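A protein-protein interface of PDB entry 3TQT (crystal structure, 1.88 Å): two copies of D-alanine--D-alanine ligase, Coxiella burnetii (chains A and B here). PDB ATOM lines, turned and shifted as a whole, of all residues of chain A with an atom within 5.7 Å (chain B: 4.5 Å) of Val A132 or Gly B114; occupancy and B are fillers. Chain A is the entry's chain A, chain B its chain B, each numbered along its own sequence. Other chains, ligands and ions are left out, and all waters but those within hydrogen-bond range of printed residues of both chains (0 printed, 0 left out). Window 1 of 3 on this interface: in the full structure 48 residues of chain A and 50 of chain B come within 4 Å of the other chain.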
ATOM      1  N   ASP A 113      31.344   1.806   8.790  1.00  0.00           N
ATOM      2  CA  ASP A 113      30.976   1.088   7.570  1.00  0.00           C
ATOM      3  C   ASP A 113      30.210   1.940   6.578  1.00  0.00           C
ATOM      4  O   ASP A 113      29.657   1.424   5.609  1.00  0.00           O
ATOM      5  CB  ASP A 113      30.178  -0.183   7.867  1.00  0.00           C
ATOM      6  CG  ASP A 113      28.885   0.084   8.627  1.00  0.00           C
ATOM      7  OD1 ASP A 113      28.468   1.256   8.789  1.00  0.00           O
ATOM      8  OD2 ASP A 113      28.284  -0.911   9.077  1.00  0.00           O
ATOM      9  N   GLY A 114      30.167   3.241   6.835  1.00  0.00           N
ATOM     10  CA  GLY A 114      29.485   4.145   5.946  1.00  0.00           C
ATOM     11  C   GLY A 114      28.040   4.406   6.298  1.00  0.00           C
ATOM     12  O   GLY A 114      27.453   5.321   5.752  1.00  0.00           O
ATOM     13  N   GLN A 117      27.833   7.730   8.283  1.00  0.00           N
ATOM     14  CA  GLN A 117      28.258   8.719   7.293  1.00  0.00           C
ATOM     15  C   GLN A 117      27.143   8.986   6.284  1.00  0.00           C
ATOM     16  O   GLN A 117      26.927  10.120   5.873  1.00  0.00           O
ATOM     17  CB  GLN A 117      29.503   8.220   6.552  1.00  0.00           C
ATOM     18  CG  GLN A 117      30.777   8.197   7.420  1.00  0.00           C
ATOM     19  CD  GLN A 117      30.799   7.044   8.434  1.00  0.00           C
ATOM     20  OE1 GLN A 117      30.128   6.031   8.253  1.00  0.00           O
ATOM     21  NE2 GLN A 117      31.586   7.198   9.488  1.00  0.00           N
ATOM     22  N   GLY A 118      26.442   7.935   5.875  1.00  0.00           N
ATOM     23  CA  GLY A 118      25.362   8.075   4.903  1.00  0.00           C
ATOM     24  C   GLY A 118      24.213   8.925   5.420  1.00  0.00           C
ATOM     25  O   GLY A 118      23.663   9.764   4.692  1.00  0.00           O
ATOM     26  N   GLU A 121      25.396  12.461   5.426  1.00  0.00           N
ATOM     27  CA  GLU A 121      25.317  13.017   4.079  1.00  0.00           C
ATOM     28  C   GLU A 121      23.884  13.423   3.755  1.00  0.00           C
ATOM     29  O   GLU A 121      23.649  14.476   3.169  1.00  0.00           O
ATOM     30  CB  GLU A 121      25.801  12.024   3.024  1.00  0.00           C
ATOM     31  CG  GLU A 121      27.268  11.691   3.115  1.00  0.00           C
ATOM     32  CD  GLU A 121      28.156  12.784   2.575  1.00  0.00           C
ATOM     33  OE1 GLU A 121      27.632  13.759   1.994  1.00  0.00           O
ATOM     34  OE2 GLU A 121      29.387  12.662   2.735  1.00  0.00           O
ATOM     35  N   TYR A 127      30.969  16.380   8.607  1.00  0.00           N
ATOM     36  CA  TYR A 127      31.354  15.391   9.600  1.00  0.00           C
ATOM     37  C   TYR A 127      32.812  14.981   9.459  1.00  0.00           C
ATOM     38  O   TYR A 127      33.393  15.005   8.360  1.00  0.00           O
ATOM     39  CB  TYR A 127      30.431  14.171   9.556  1.00  0.00           C
ATOM     40  CG  TYR A 127      30.450  13.422   8.253  1.00  0.00           C
ATOM     41  CD1 TYR A 127      31.316  12.344   8.060  1.00  0.00           C
ATOM     42  CD2 TYR A 127      29.588  13.772   7.223  1.00  0.00           C
ATOM     43  CE1 TYR A 127      31.331  11.653   6.880  1.00  0.00           C
ATOM     44  CE2 TYR A 127      29.598  13.083   6.024  1.00  0.00           C
ATOM     45  CZ  TYR A 127      30.462  12.023   5.862  1.00  0.00           C
ATOM     46  OH  TYR A 127      30.465  11.351   4.673  1.00  0.00           O
ATOM     47  N   ALA A 130      36.349   9.737   7.220  1.00  0.00           N
ATOM     48  CA  ALA A 130      36.131   9.133   5.923  1.00  0.00           C
ATOM     49  C   ALA A 130      34.690   9.296   5.510  1.00  0.00           C
ATOM     50  O   ALA A 130      33.805   9.190   6.350  1.00  0.00           O
ATOM     51  CB  ALA A 130      36.479   7.654   5.996  1.00  0.00           C
ATOM     52  N   ASN A 131      34.458   9.558   4.224  1.00  0.00           N
ATOM     53  CA  ASN A 131      33.102   9.641   3.696  1.00  0.00           C
ATOM     54  C   ASN A 131      32.485   8.248   3.535  1.00  0.00           C
ATOM     55  O   ASN A 131      33.059   7.272   3.992  1.00  0.00           O
ATOM     56  CB  ASN A 131      33.039  10.444   2.392  1.00  0.00           C
ATOM     57  CG  ASN A 131      33.680   9.725   1.211  1.00  0.00           C
ATOM     58  OD1 ASN A 131      34.208   8.621   1.337  1.00  0.00           O
ATOM     59  ND2 ASN A 131      33.614  10.356   0.041  1.00  0.00           N
ATOM     60  N   VAL A 132      31.328   8.159   2.893  1.00  0.00           N
ATOM     61  CA  VAL A 132      30.635   6.877   2.817  1.00  0.00           C
ATOM     62  C   VAL A 132      31.452   5.858   2.039  1.00  0.00           C
ATOM     63  O   VAL A 132      31.656   4.735   2.489  1.00  0.00           O
ATOM     64  CB  VAL A 132      29.236   7.008   2.186  1.00  0.00           C
ATOM     65  CG1 VAL A 132      28.663   5.620   1.875  1.00  0.00           C
ATOM     66  CG2 VAL A 132      28.314   7.783   3.125  1.00  0.00           C
ATOM     67  N   GLN A 133      31.923   6.255   0.865  1.00  0.00           N
ATOM     68  CA  GLN A 133      32.673   5.340   0.027  1.00  0.00           C
ATOM     69  C   GLN A 133      33.964   4.869   0.670  1.00  0.00           C
ATOM     70  O   GLN A 133      34.310   3.694   0.606  1.00  0.00           O
ATOM     71  CB  GLN A 133      33.008   5.977  -1.319  1.00  0.00           C
ATOM     72  CG  GLN A 133      34.014   5.148  -2.121  1.00  0.00           C
ATOM     73  CD  GLN A 133      34.869   6.004  -3.037  1.00  0.00           C
ATOM     74  OE1 GLN A 133      35.965   6.409  -2.678  1.00  0.00           O
ATOM     75  NE2 GLN A 133      34.358   6.293  -4.221  1.00  0.00           N
ATOM     76  N   SER A 134      34.691   5.797   1.267  1.00  0.00           N
ATOM     77  CA  SER A 134      35.987   5.483   1.848  1.00  0.00           C
ATOM     78  C   SER A 134      35.807   4.631   3.100  1.00  0.00           C
ATOM     79  O   SER A 134      36.595   3.736   3.371  1.00  0.00           O
ATOM     80  CB  SER A 134      36.754   6.767   2.192  1.00  0.00           C
ATOM     81  OG  SER A 134      38.090   6.436   2.525  1.00  0.00           O
ATOM     82  N   SER A 135      34.776   4.933   3.878  1.00  0.00           N
ATOM     83  CA  SER A 135      34.476   4.126   5.057  1.00  0.00           C
ATOM     84  C   SER A 135      34.191   2.682   4.620  1.00  0.00           C
ATOM     85  O   SER A 135      34.678   1.734   5.225  1.00  0.00           O
ATOM     86  CB  SER A 135      33.263   4.690   5.798  1.00  0.00           C
ATOM     87  OG  SER A 135      33.532   6.001   6.274  1.00  0.00           O
ATOM     88  N   ALA A 136      33.388   2.530   3.570  1.00  0.00           N
ATOM     89  CA  ALA A 136      32.983   1.199   3.117  1.00  0.00           C
ATOM     90  C   ALA A 136      34.179   0.450   2.573  1.00  0.00           C
ATOM     91  O   ALA A 136      34.378  -0.726   2.871  1.00  0.00           O
ATOM     92  CB  ALA A 136      31.879   1.294   2.080  1.00  0.00           C
ATOM     93  N   VAL A 137      34.997   1.131   1.786  1.00  0.00           N
ATOM     94  CA  VAL A 137      36.201   0.503   1.261  1.00  0.00           C
ATOM     95  C   VAL A 137      37.174   0.060   2.368  1.00  0.00           C
ATOM     96  O   VAL A 137      37.753  -1.025   2.299  1.00  0.00           O
ATOM     97  CB  VAL A 137      36.923   1.413   0.247  1.00  0.00           C
ATOM     98  CG1 VAL A 137      38.314   0.881  -0.068  1.00  0.00           C
ATOM     99  CG2 VAL A 137      36.098   1.529  -1.024  1.00  0.00           C
ATOM    100  N   GLU B 112      22.213   6.020  -4.991  1.00  0.00           N
ATOM    101  CA  GLU B 112      22.996   4.866  -5.415  1.00  0.00           C
ATOM    102  C   GLU B 112      24.386   4.881  -4.818  1.00  0.00           C
ATOM    103  O   GLU B 112      25.213   4.033  -5.158  1.00  0.00           O
ATOM    104  CB  GLU B 112      23.154   4.864  -6.934  1.00  0.00           C
ATOM    105  CG  GLU B 112      21.922   4.453  -7.678  1.00  0.00           C
ATOM    106  CD  GLU B 112      22.116   4.505  -9.177  1.00  0.00           C
ATOM    107  OE1 GLU B 112      22.536   3.478  -9.763  1.00  0.00           O
ATOM    108  OE2 GLU B 112      21.840   5.572  -9.760  1.00  0.00           O
ATOM    109  N   ASP B 113      24.649   5.843  -3.938  1.00  0.00           N
ATOM    110  CA  ASP B 113      26.018   6.086  -3.478  1.00  0.00           C
ATOM    111  C   ASP B 113      26.224   5.703  -2.029  1.00  0.00           C
ATOM    112  O   ASP B 113      27.219   6.082  -1.408  1.00  0.00           O
ATOM    113  CB  ASP B 113      26.424   7.539  -3.696  1.00  0.00           C
ATOM    114  CG  ASP B 113      25.679   8.513  -2.786  1.00  0.00           C
ATOM    115  OD1 ASP B 113      24.808   8.106  -1.973  1.00  0.00           O
ATOM    116  OD2 ASP B 113      25.967   9.714  -2.912  1.00  0.00           O
ATOM    117  N   GLY B 114      25.276   4.940  -1.502  1.00  0.00           N
ATOM    118  CA  GLY B 114      25.446   4.316  -0.211  1.00  0.00           C
ATOM    119  C   GLY B 114      24.839   5.098   0.924  1.00  0.00           C
ATOM    120  O   GLY B 114      24.655   4.554   2.005  1.00  0.00           O
ATOM    121  N   ALA B 115      24.563   6.382   0.702  1.00  0.00           N
ATOM    122  CA  ALA B 115      24.070   7.211   1.795  1.00  0.00           C
ATOM    123  C   ALA B 115      22.692   6.758   2.233  1.00  0.00           C
ATOM    124  O   ALA B 115      22.462   6.501   3.415  1.00  0.00           O
ATOM    125  CB  ALA B 115      24.080   8.692   1.417  1.00  0.00           C
ATOM    126  N   LEU B 116      21.773   6.635   1.276  1.00  0.00           N
ATOM    127  CA  LEU B 116      20.437   6.167   1.591  1.00  0.00           C
ATOM    128  C   LEU B 116      20.481   4.743   2.153  1.00  0.00           C
ATOM    129  O   LEU B 116      19.796   4.443   3.123  1.00  0.00           O
ATOM    130  CB  LEU B 116      19.535   6.238   0.351  1.00  0.00           C
ATOM    131  CG  LEU B 116      18.022   6.345   0.527  1.00  0.00           C
ATOM    132  CD1 LEU B 116      17.619   7.448   1.522  1.00  0.00           C
ATOM    133  CD2 LEU B 116      17.373   6.598  -0.839  1.00  0.00           C
ATOM    134  N   GLN B 117      21.272   3.872   1.535  1.00  0.00           N
ATOM    135  CA  GLN B 117      21.472   2.515   2.053  1.00  0.00           C
ATOM    136  C   GLN B 117      21.977   2.538   3.499  1.00  0.00           C
ATOM    137  O   GLN B 117      21.544   1.747   4.343  1.00  0.00           O
ATOM    138  CB  GLN B 117      22.463   1.745   1.172  1.00  0.00           C
ATOM    139  CG  GLN B 117      21.931   1.414  -0.234  1.00  0.00           C
ATOM    140  CD  GLN B 117      21.774   2.641  -1.120  1.00  0.00           C
ATOM    141  OE1 GLN B 117      22.449   3.670  -0.928  1.00  0.00           O
ATOM    142  NE2 GLN B 117      20.885   2.540  -2.099  1.00  0.00           N
ATOM    143  N   GLY B 118      22.903   3.447   3.775  1.00  0.00           N
ATOM    144  CA  GLY B 118      23.426   3.624   5.121  1.00  0.00           C
ATOM    145  C   GLY B 118      22.346   3.911   6.145  1.00  0.00           C
ATOM    146  O   GLY B 118      22.327   3.329   7.246  1.00  0.00           O
ATOM    147  N   VAL B 132      25.519  -0.747   1.265  1.00  0.00           N
ATOM    148  CA  VAL B 132      26.277   0.498   1.294  1.00  0.00           C
ATOM    149  C   VAL B 132      27.555   0.345   0.468  1.00  0.00           C
ATOM    150  O   VAL B 132      27.848   1.143  -0.428  1.00  0.00           O
ATOM    151  CB  VAL B 132      26.625   0.865   2.734  1.00  0.00           C
ATOM    152  CG1 VAL B 132      27.670   1.996   2.781  1.00  0.00           C
ATOM    153  CG2 VAL B 132      25.360   1.269   3.466  1.00  0.00           C
ATOM    154  N   SER B 135      26.953  -0.290  -3.339  1.00  0.00           N
ATOM    155  CA  SER B 135      26.525   0.995  -3.895  1.00  0.00           C
ATOM    156  C   SER B 135      27.708   1.958  -4.069  1.00  0.00           C
ATOM    157  O   SER B 135      27.897   2.560  -5.126  1.00  0.00           O
ATOM    158  CB  SER B 135      25.451   1.640  -3.009  1.00  0.00           C
ATOM    159  OG  SER B 135      24.296   0.822  -2.923  1.00  0.00           O
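OD1 of Asp B113 is in hydrogen-bond range of N of Ala B115, at 3.2 Å. N of Gly B114 lies close to OE1 of Gln B117 (3.2 Å).
Val B132 touches Asp A113. Gly A118 touches Ala B115 (O to CB, 3.5 Å). Asp B113 touches Val A132. Val A132 touches Gly B114 (CG1 to C, 3.97 Å). Val B132 touches Val A132 (CG1 to CG1, 3.9 Å).
Val A132 touches just these residues of chain B: Asp B113 (3.6 Å), Gly B114 (3.97 Å) and Val B132 (3.9 Å). Printed residues of chain A within 4 Å of Gly B114: Val A132. Printed residues of chain B within 4 Å of Asp A113: Val B132. Printed residues of chain A within 4 Å of Asp B113: Val A132 (3.6 Å). Of the printed residues of chain A, Val B132 touches Asp A113 and Val A132. Ala A136 touches none of the printed residues of chain B. The nearest residue of chain B that does not touch Val A132 is Ala B115 (4.3 Å). The nearest printed residue of chain B that does not touch Asp A113 is Gly B118 (6.6 Å).
Of the 14 printed residues of chain A, 3 touch a printed residue of chain B. Hydrophobic or aromatic side chains of chain B that line the printed part of chain A: Ala B115 and Val B132. Among the printed residues, 5 pairs touch across the chains.
Asp A113 touches Val B132, and with the chains exchanged Val A132 touches Asp B113. Val A132 touches Gly B114, but with the chains exchanged Gly A114 does not touch Val B132 (4.2 Å). Val A132 touches its own counterpart, Val B132. Positions printed for both chains: 113, 114, 117, 118, 132 and 135. Of the 5 pairs that touch across the chains among the printed residues, 3 have their exchanged pair printed and touching as well.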
